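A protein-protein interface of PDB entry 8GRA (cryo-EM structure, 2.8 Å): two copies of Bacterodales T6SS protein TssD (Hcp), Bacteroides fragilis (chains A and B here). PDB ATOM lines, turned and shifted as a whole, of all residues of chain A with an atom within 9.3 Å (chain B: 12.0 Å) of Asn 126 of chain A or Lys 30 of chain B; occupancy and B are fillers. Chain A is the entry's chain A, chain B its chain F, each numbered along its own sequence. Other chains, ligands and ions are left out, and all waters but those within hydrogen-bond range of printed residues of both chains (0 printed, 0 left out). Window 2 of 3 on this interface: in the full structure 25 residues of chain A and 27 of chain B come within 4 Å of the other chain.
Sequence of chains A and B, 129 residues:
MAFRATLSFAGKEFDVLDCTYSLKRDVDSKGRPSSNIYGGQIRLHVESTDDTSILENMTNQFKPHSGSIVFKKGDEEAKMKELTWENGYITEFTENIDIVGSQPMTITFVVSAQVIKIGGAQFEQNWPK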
ATOM      1  N   ASN A  36      18.698  16.920 -21.594  1.00  0.00           N
ATOM      2  CA  ASN A  36      18.171  16.415 -22.851  1.00  0.00           C
ATOM      3  C   ASN A  36      17.483  15.071 -22.620  1.00  0.00           C
ATOM      4  O   ASN A  36      17.414  14.560 -21.501  1.00  0.00           O
ATOM      5  CB  ASN A  36      19.284  16.302 -23.896  1.00  0.00           C
ATOM      6  CG  ASN A  36      20.479  15.519 -23.395  1.00  0.00           C
ATOM      7  OD1 ASN A  36      20.616  15.266 -22.202  1.00  0.00           O
ATOM      8  ND2 ASN A  36      21.353  15.129 -24.312  1.00  0.00           N
ATOM      9  N   ILE A  37      16.970  14.492 -23.698  1.00  0.00           N
ATOM     10  CA  ILE A  37      16.186  13.267 -23.610  1.00  0.00           C
ATOM     11  C   ILE A  37      17.122  12.073 -23.491  1.00  0.00           C
ATOM     12  O   ILE A  37      18.121  11.976 -24.213  1.00  0.00           O
ATOM     13  CB  ILE A  37      15.259  13.131 -24.826  1.00  0.00           C
ATOM     14  CG1 ILE A  37      14.384  14.373 -24.964  1.00  0.00           C
ATOM     15  CG2 ILE A  37      14.396  11.897 -24.709  1.00  0.00           C
ATOM     16  CD1 ILE A  37      13.675  14.467 -26.279  1.00  0.00           C
ATOM     17  N   TYR A  38      16.808  11.165 -22.571  1.00  0.00           N
ATOM     18  CA  TYR A  38      17.558   9.928 -22.424  1.00  0.00           C
ATOM     19  C   TYR A  38      16.592   8.782 -22.171  1.00  0.00           C
ATOM     20  O   TYR A  38      15.447   8.984 -21.763  1.00  0.00           O
ATOM     21  CB  TYR A  38      18.601  10.015 -21.300  1.00  0.00           C
ATOM     22  CG  TYR A  38      18.049  10.388 -19.950  1.00  0.00           C
ATOM     23  CD1 TYR A  38      17.884  11.714 -19.591  1.00  0.00           C
ATOM     24  CD2 TYR A  38      17.707   9.416 -19.027  1.00  0.00           C
ATOM     25  CE1 TYR A  38      17.386  12.060 -18.361  1.00  0.00           C
ATOM     26  CE2 TYR A  38      17.206   9.756 -17.795  1.00  0.00           C
ATOM     27  CZ  TYR A  38      17.049  11.080 -17.468  1.00  0.00           C
ATOM     28  OH  TYR A  38      16.552  11.430 -16.240  1.00  0.00           O
ATOM     29  N   GLY A  39      17.071   7.564 -22.428  1.00  0.00           N
ATOM     30  CA  GLY A  39      16.265   6.364 -22.328  1.00  0.00           C
ATOM     31  C   GLY A  39      16.280   5.594 -23.639  1.00  0.00           C
ATOM     32  O   GLY A  39      17.301   5.550 -24.335  1.00  0.00           O
ATOM     33  N   GLY A  40      15.144   4.998 -23.973  1.00  0.00           N
ATOM     34  CA  GLY A  40      14.982   4.340 -25.250  1.00  0.00           C
ATOM     35  C   GLY A  40      15.138   2.838 -25.251  1.00  0.00           C
ATOM     36  O   GLY A  40      15.275   2.254 -26.328  1.00  0.00           O
ATOM     37  N   GLN A  41      15.147   2.197 -24.087  1.00  0.00           N
ATOM     38  CA  GLN A  41      15.231   0.746 -24.035  1.00  0.00           C
ATOM     39  C   GLN A  41      13.880   0.122 -24.351  1.00  0.00           C
ATOM     40  O   GLN A  41      12.827   0.699 -24.074  1.00  0.00           O
ATOM     41  CB  GLN A  41      15.710   0.291 -22.662  1.00  0.00           C
ATOM     42  CG  GLN A  41      17.146   0.661 -22.357  1.00  0.00           C
ATOM     43  CD  GLN A  41      17.610   0.110 -21.028  1.00  0.00           C
ATOM     44  OE1 GLN A  41      16.832   0.018 -20.078  1.00  0.00           O
ATOM     45  NE2 GLN A  41      18.880  -0.264 -20.952  1.00  0.00           N
ATOM     46  N   ASN A  87      21.188  -1.681 -34.819  1.00  0.00           N
ATOM     47  CA  ASN A  87      22.456  -1.536 -34.101  1.00  0.00           C
ATOM     48  C   ASN A  87      22.258  -1.625 -32.585  1.00  0.00           C
ATOM     49  O   ASN A  87      22.598  -0.714 -31.832  1.00  0.00           O
ATOM     50  CB  ASN A  87      23.151  -0.227 -34.489  1.00  0.00           C
ATOM     51  CG  ASN A  87      24.644  -0.281 -34.297  1.00  0.00           C
ATOM     52  OD1 ASN A  87      25.175  -1.249 -33.762  1.00  0.00           O
ATOM     53  ND2 ASN A  87      25.334   0.763 -34.732  1.00  0.00           N
ATOM     54  N   SER A 112      19.039  -2.685 -26.024  1.00  0.00           N
ATOM     55  CA  SER A 112      19.619  -1.344 -26.041  1.00  0.00           C
ATOM     56  C   SER A 112      20.143  -1.060 -27.445  1.00  0.00           C
ATOM     57  O   SER A 112      21.145  -1.645 -27.864  1.00  0.00           O
ATOM     58  CB  SER A 112      20.733  -1.222 -25.007  1.00  0.00           C
ATOM     59  OG  SER A 112      20.250  -1.487 -23.704  1.00  0.00           O
ATOM     60  N   ALA A 113      19.486  -0.148 -28.158  1.00  0.00           N
ATOM     61  CA  ALA A 113      19.772   0.110 -29.561  1.00  0.00           C
ATOM     62  C   ALA A 113      20.169   1.563 -29.780  1.00  0.00           C
ATOM     63  O   ALA A 113      19.866   2.445 -28.974  1.00  0.00           O
ATOM     64  CB  ALA A 113      18.567  -0.232 -30.444  1.00  0.00           C
ATOM     65  N   GLN A 114      20.870   1.805 -30.889  1.00  0.00           N
ATOM     66  CA  GLN A 114      21.273   3.166 -31.220  1.00  0.00           C
ATOM     67  C   GLN A 114      20.116   3.978 -31.793  1.00  0.00           C
ATOM     68  O   GLN A 114      19.993   5.172 -31.506  1.00  0.00           O
ATOM     69  CB  GLN A 114      22.448   3.152 -32.191  1.00  0.00           C
ATOM     70  CG  GLN A 114      23.124   4.501 -32.314  1.00  0.00           C
ATOM     71  CD  GLN A 114      24.079   4.582 -33.481  1.00  0.00           C
ATOM     72  OE1 GLN A 114      24.295   3.605 -34.194  1.00  0.00           O
ATOM     73  NE2 GLN A 114      24.658   5.755 -33.685  1.00  0.00           N
ATOM     74  N   VAL A 115      19.272   3.362 -32.621  1.00  0.00           N
ATOM     75  CA  VAL A 115      18.140   4.040 -33.241  1.00  0.00           C
ATOM     76  C   VAL A 115      16.880   3.215 -33.021  1.00  0.00           C
ATOM     77  O   VAL A 115      16.905   1.986 -33.143  1.00  0.00           O
ATOM     78  CB  VAL A 115      18.359   4.275 -34.751  1.00  0.00           C
ATOM     79  CG1 VAL A 115      17.638   5.532 -35.200  1.00  0.00           C
ATOM     80  CG2 VAL A 115      19.828   4.356 -35.082  1.00  0.00           C
ATOM     81  N   PHE A 123      14.098   8.296 -32.627  1.00  0.00           N
ATOM     82  CA  PHE A 123      15.021   8.751 -31.599  1.00  0.00           C
ATOM     83  C   PHE A 123      16.372   8.101 -31.842  1.00  0.00           C
ATOM     84  O   PHE A 123      16.453   6.882 -32.008  1.00  0.00           O
ATOM     85  CB  PHE A 123      14.507   8.403 -30.197  1.00  0.00           C
ATOM     86  CG  PHE A 123      15.404   8.870 -29.090  1.00  0.00           C
ATOM     87  CD1 PHE A 123      15.598  10.215 -28.852  1.00  0.00           C
ATOM     88  CD2 PHE A 123      16.061   7.955 -28.290  1.00  0.00           C
ATOM     89  CE1 PHE A 123      16.428  10.637 -27.839  1.00  0.00           C
ATOM     90  CE2 PHE A 123      16.890   8.374 -27.274  1.00  0.00           C
ATOM     91  CZ  PHE A 123      17.074   9.716 -27.051  1.00  0.00           C
ATOM     92  N   GLU A 124      17.427   8.907 -31.858  1.00  0.00           N
ATOM     93  CA  GLU A 124      18.768   8.417 -32.128  1.00  0.00           C
ATOM     94  C   GLU A 124      19.734   8.926 -31.069  1.00  0.00           C
ATOM     95  O   GLU A 124      19.676  10.091 -30.671  1.00  0.00           O
ATOM     96  CB  GLU A 124      19.230   8.851 -33.520  1.00  0.00           C
ATOM     97  CG  GLU A 124      20.699   8.637 -33.791  1.00  0.00           C
ATOM     98  CD  GLU A 124      21.019   8.623 -35.270  1.00  0.00           C
ATOM     99  OE1 GLU A 124      20.634   9.581 -35.971  1.00  0.00           O
ATOM    100  OE2 GLU A 124      21.658   7.656 -35.732  1.00  0.00           O
ATOM    101  N   GLN A 125      20.609   8.042 -30.610  1.00  0.00           N
ATOM    102  CA  GLN A 125      21.715   8.400 -29.735  1.00  0.00           C
ATOM    103  C   GLN A 125      23.003   8.490 -30.543  1.00  0.00           C
ATOM    104  O   GLN A 125      23.146   7.868 -31.597  1.00  0.00           O
ATOM    105  CB  GLN A 125      21.876   7.372 -28.614  1.00  0.00           C
ATOM    106  CG  GLN A 125      20.902   7.533 -27.471  1.00  0.00           C
ATOM    107  CD  GLN A 125      20.583   6.218 -26.807  1.00  0.00           C
ATOM    108  OE1 GLN A 125      20.729   5.159 -27.409  1.00  0.00           O
ATOM    109  NE2 GLN A 125      20.148   6.275 -25.558  1.00  0.00           N
ATOM    110  N   ASN A 126      23.948   9.274 -30.041  1.00  0.00           N
ATOM    111  CA  ASN A 126      25.262   9.370 -30.662  1.00  0.00           C
ATOM    112  C   ASN A 126      26.236   8.440 -29.947  1.00  0.00           C
ATOM    113  O   ASN A 126      26.281   8.398 -28.715  1.00  0.00           O
ATOM    114  CB  ASN A 126      25.760  10.823 -30.707  1.00  0.00           C
ATOM    115  CG  ASN A 126      25.883  11.481 -29.336  1.00  0.00           C
ATOM    116  OD1 ASN A 126      26.279  10.869 -28.352  1.00  0.00           O
ATOM    117  ND2 ASN A 126      25.536  12.761 -29.279  1.00  0.00           N
ATOM    118  N   TRP A 127      26.963   7.648 -30.727  1.00  0.00           N
ATOM    119  CA  TRP A 127      27.898   6.672 -30.194  1.00  0.00           C
ATOM    120  C   TRP A 127      29.283   6.997 -30.734  1.00  0.00           C
ATOM    121  O   TRP A 127      29.493   6.942 -31.957  1.00  0.00           O
ATOM    122  CB  TRP A 127      27.478   5.244 -30.566  1.00  0.00           C
ATOM    123  CG  TRP A 127      26.368   4.695 -29.703  1.00  0.00           C
ATOM    124  CD1 TRP A 127      25.604   5.388 -28.817  1.00  0.00           C
ATOM    125  CD2 TRP A 127      25.907   3.338 -29.647  1.00  0.00           C
ATOM    126  NE1 TRP A 127      24.698   4.557 -28.214  1.00  0.00           N
ATOM    127  CE2 TRP A 127      24.863   3.291 -28.706  1.00  0.00           C
ATOM    128  CE3 TRP A 127      26.278   2.157 -30.299  1.00  0.00           C
ATOM    129  CZ2 TRP A 127      24.186   2.114 -28.399  1.00  0.00           C
ATOM    130  CZ3 TRP A 127      25.603   0.992 -29.993  1.00  0.00           C
ATOM    131  CH2 TRP A 127      24.571   0.978 -29.053  1.00  0.00           C
ATOM    132  N   PRO A 128      30.248   7.339 -29.881  1.00  0.00           N
ATOM    133  CA  PRO A 128      31.535   7.838 -30.380  1.00  0.00           C
ATOM    134  C   PRO A 128      32.431   6.744 -30.939  1.00  0.00           C
ATOM    135  O   PRO A 128      33.313   6.235 -30.242  1.00  0.00           O
ATOM    136  CB  PRO A 128      32.153   8.484 -29.137  1.00  0.00           C
ATOM    137  CG  PRO A 128      31.583   7.712 -28.000  1.00  0.00           C
ATOM    138  CD  PRO A 128      30.204   7.276 -28.411  1.00  0.00           C
ATOM    139  N   LYS A 129      32.213   6.376 -32.197  1.00  0.00           N
ATOM    140  CA  LYS A 129      33.069   5.399 -32.856  1.00  0.00           C
ATOM    141  C   LYS A 129      33.723   6.008 -34.091  1.00  0.00           C
ATOM    142  O   LYS A 129      34.847   6.510 -34.027  1.00  0.00           O
ATOM    143  CB  LYS A 129      32.272   4.149 -33.235  1.00  0.00           C
ATOM    144  CG  LYS A 129      33.126   2.901 -33.439  1.00  0.00           C
ATOM    145  CD  LYS A 129      32.265   1.676 -33.712  1.00  0.00           C
ATOM    146  CE  LYS A 129      33.084   0.397 -33.651  1.00  0.00           C
ATOM    147  NZ  LYS A 129      32.248  -0.782 -33.283  1.00  0.00           N
ATOM    148  N   ARG B  25      24.073  -7.390 -18.271  1.00  0.00           N
ATOM    149  CA  ARG B  25      25.240  -6.592 -18.632  1.00  0.00           C
ATOM    150  C   ARG B  25      25.027  -5.161 -18.165  1.00  0.00           C
ATOM    151  O   ARG B  25      23.893  -4.689 -18.072  1.00  0.00           O
ATOM    152  CB  ARG B  25      25.492  -6.581 -20.142  1.00  0.00           C
ATOM    153  CG  ARG B  25      25.875  -7.907 -20.734  1.00  0.00           C
ATOM    154  CD  ARG B  25      26.079  -7.785 -22.223  1.00  0.00           C
ATOM    155  NE  ARG B  25      27.405  -7.282 -22.553  1.00  0.00           N
ATOM    156  CZ  ARG B  25      27.887  -7.199 -23.784  1.00  0.00           C
ATOM    157  NH1 ARG B  25      27.175  -7.577 -24.831  1.00  0.00           N
ATOM    158  NH2 ARG B  25      29.112  -6.719 -23.970  1.00  0.00           N
ATOM    159  N   ASP B  26      26.125  -4.465 -17.885  1.00  0.00           N
ATOM    160  CA  ASP B  26      26.066  -3.065 -17.484  1.00  0.00           C
ATOM    161  C   ASP B  26      26.027  -2.166 -18.710  1.00  0.00           C
ATOM    162  O   ASP B  26      26.646  -2.454 -19.734  1.00  0.00           O
ATOM    163  CB  ASP B  26      27.260  -2.693 -16.607  1.00  0.00           C
ATOM    164  CG  ASP B  26      27.114  -3.191 -15.187  1.00  0.00           C
ATOM    165  OD1 ASP B  26      26.082  -3.819 -14.881  1.00  0.00           O
ATOM    166  OD2 ASP B  26      28.031  -2.958 -14.375  1.00  0.00           O
ATOM    167  N   VAL B  27      25.294  -1.063 -18.595  1.00  0.00           N
ATOM    168  CA  VAL B  27      24.994  -0.204 -19.732  1.00  0.00           C
ATOM    169  C   VAL B  27      25.400   1.225 -19.398  1.00  0.00           C
ATOM    170  O   VAL B  27      25.090   1.730 -18.315  1.00  0.00           O
ATOM    171  CB  VAL B  27      23.505  -0.286 -20.121  1.00  0.00           C
ATOM    172  CG1 VAL B  27      23.016   1.010 -20.715  1.00  0.00           C
ATOM    173  CG2 VAL B  27      23.294  -1.412 -21.105  1.00  0.00           C
ATOM    174  N   ASP B  28      26.104   1.862 -20.327  1.00  0.00           N
ATOM    175  CA  ASP B  28      26.562   3.234 -20.183  1.00  0.00           C
ATOM    176  C   ASP B  28      25.373   4.200 -20.202  1.00  0.00           C
ATOM    177  O   ASP B  28      24.257   3.846 -20.586  1.00  0.00           O
ATOM    178  CB  ASP B  28      27.564   3.543 -21.300  1.00  0.00           C
ATOM    179  CG  ASP B  28      27.869   5.008 -21.438  1.00  0.00           C
ATOM    180  OD1 ASP B  28      27.998   5.686 -20.400  1.00  0.00           O
ATOM    181  OD2 ASP B  28      27.974   5.482 -22.588  1.00  0.00           O
ATOM    182  N   SER B  29      25.623   5.435 -19.759  1.00  0.00           N
ATOM    183  CA  SER B  29      24.565   6.442 -19.692  1.00  0.00           C
ATOM    184  C   SER B  29      23.915   6.686 -21.047  1.00  0.00           C
ATOM    185  O   SER B  29      22.759   7.119 -21.110  1.00  0.00           O
ATOM    186  CB  SER B  29      25.127   7.754 -19.152  1.00  0.00           C
ATOM    187  OG  SER B  29      25.776   8.479 -20.183  1.00  0.00           O
ATOM    188  N   LYS B  30      24.636   6.431 -22.136  1.00  0.00           N
ATOM    189  CA  LYS B  30      24.121   6.621 -23.482  1.00  0.00           C
ATOM    190  C   LYS B  30      23.600   5.331 -24.101  1.00  0.00           C
ATOM    191  O   LYS B  30      23.313   5.304 -25.298  1.00  0.00           O
ATOM    192  CB  LYS B  30      25.201   7.230 -24.372  1.00  0.00           C
ATOM    193  CG  LYS B  30      24.974   8.689 -24.695  1.00  0.00           C
ATOM    194  CD  LYS B  30      26.207   9.309 -25.322  1.00  0.00           C
ATOM    195  CE  LYS B  30      26.267  10.799 -25.039  1.00  0.00           C
ATOM    196  NZ  LYS B  30      24.919  11.426 -25.084  1.00  0.00           N
ATOM    197  N   GLY B  31      23.485   4.260 -23.317  1.00  0.00           N
ATOM    198  CA  GLY B  31      22.918   3.017 -23.784  1.00  0.00           C
ATOM    199  C   GLY B  31      23.908   2.002 -24.311  1.00  0.00           C
ATOM    200  O   GLY B  31      23.513   0.862 -24.578  1.00  0.00           O
ATOM    201  N   ARG B  32      25.166   2.371 -24.472  1.00  0.00           N
ATOM    202  CA  ARG B  32      26.171   1.439 -24.964  1.00  0.00           C
ATOM    203  C   ARG B  32      26.573   0.467 -23.858  1.00  0.00           C
ATOM    204  O   ARG B  32      26.788   0.892 -22.721  1.00  0.00           O
ATOM    205  CB  ARG B  32      27.390   2.201 -25.463  1.00  0.00           C
ATOM    206  CG  ARG B  32      28.213   1.456 -26.480  1.00  0.00           C
ATOM    207  CD  ARG B  32      29.148   2.399 -27.200  1.00  0.00           C
ATOM    208  NE  ARG B  32      29.541   1.880 -28.503  1.00  0.00           N
ATOM    209  CZ  ARG B  32      30.470   2.427 -29.273  1.00  0.00           C
ATOM    210  NH1 ARG B  32      31.127   3.511 -28.897  1.00  0.00           N
ATOM    211  NH2 ARG B  32      30.746   1.871 -30.448  1.00  0.00           N
ATOM    212  N   PRO B  33      26.667  -0.832 -24.141  1.00  0.00           N
ATOM    213  CA  PRO B  33      27.123  -1.775 -23.111  1.00  0.00           C
ATOM    214  C   PRO B  33      28.555  -1.486 -22.682  1.00  0.00           C
ATOM    215  O   PRO B  33      29.409  -1.132 -23.495  1.00  0.00           O
ATOM    216  CB  PRO B  33      27.003  -3.140 -23.797  1.00  0.00           C
ATOM    217  CG  PRO B  33      26.939  -2.846 -25.247  1.00  0.00           C
ATOM    218  CD  PRO B  33      26.288  -1.514 -25.387  1.00  0.00           C
ATOM    219  N   SER B  34      28.814  -1.648 -21.386  1.00  0.00           N
ATOM    220  CA  SER B  34      30.116  -1.319 -20.819  1.00  0.00           C
ATOM    221  C   SER B  34      30.560  -2.386 -19.831  1.00  0.00           C
ATOM    222  O   SER B  34      31.133  -2.084 -18.782  1.00  0.00           O
ATOM    223  CB  SER B  34      30.093   0.054 -20.155  1.00  0.00           C
ATOM    224  OG  SER B  34      29.465   0.000 -18.891  1.00  0.00           O
ATOM    225  N   SER B  35      30.314  -3.647 -20.158  1.00  0.00           N
ATOM    226  CA  SER B  35      30.681  -4.760 -19.292  1.00  0.00           C
ATOM    227  C   SER B  35      30.558  -6.045 -20.098  1.00  0.00           C
ATOM    228  O   SER B  35      30.162  -6.033 -21.267  1.00  0.00           O
ATOM    229  CB  SER B  35      29.804  -4.799 -18.040  1.00  0.00           C
ATOM    230  OG  SER B  35      29.874  -6.056 -17.395  1.00  0.00           O
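The backbone carbonyl oxygen of Ala 113 of chain A sits close to the side-chain amide oxygen of Gln 125 of chain A (3.2 Å).
The backbone NH (N) of Gln 125 of chain A is in hydrogen-bond range of the backbone carbonyl oxygen (O) of Gln 114 of chain A.
OG of Ser 112 of chain A sits at hydrogen-bond distance from NE2 of Gln 41 of chain A (3.3 Å).
O of Gly 39 of chain A lies within hydrogen-bond range of NE2 of Gln 125 of chain A, 3.2 Å away.
CB of Ser 112 of chain A touches O of Gly 31 of chain B (3.5 Å).
Asn 126 of chain A touches Lys 30 of chain B.
Trp 127 of chain A touches Arg 32 of chain B (CE3 to NE, 3.7 Å).
Arg 32 of chain B touches Pro 128 of chain A.
Lys 129 of chain A touches Arg 32 of chain B.
Hydrophobic or aromatic side chains of chain A that line the printed part of chain B: Trp 127 and Pro 128.
No position is printed for both chains.
Of the 7 pairs that touch across the chains among the printed residues, none has its exchanged pair printed and touching as well.
The backbone carbonyl oxygen (O) of Lys 30 of chain B is in hydrogen-bond range of the indole nitrogen (NE1) of Trp 127 of chain A (3.3 Å).
O of Lys 30 of chain B lies close to NE2 of Gln 125 of chain A, 3.3 Å away.
Asn 126 of chain A touches just one residue of chain B: Lys 30.
No residue of chain B comes within 4 Å of Gly 39 of chain A.
No residue of chain B comes within 4 Å of Glu 124 of chain A.
Of chain B, only Lys 30 comes within 4 Å of Gln 125 of chain A.
Pro 128 of chain A touches just one residue of chain B: Arg 32 (3.7 Å).
No residue of chain A comes within 4 Å of Asp 28 of chain B.
Gly 31 of chain B touches one residue of chain A.
Printed residues of chain B within 4 Å of Ser 112 of chain A: Gly 31 (3.5 Å).
Of the printed residues of chain B, Lys 129 of chain A touches Arg 32.
Gln 41 of chain A touches none of the printed residues of chain B.
The nearest residue of chain A that does not touch Lys 30 of chain B is Asn 36 of chain A (5.2 Å).
The nearest printed residue of chain B that does not touch Ser 112 of chain A is Val 27 of chain B (4.003 Å).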
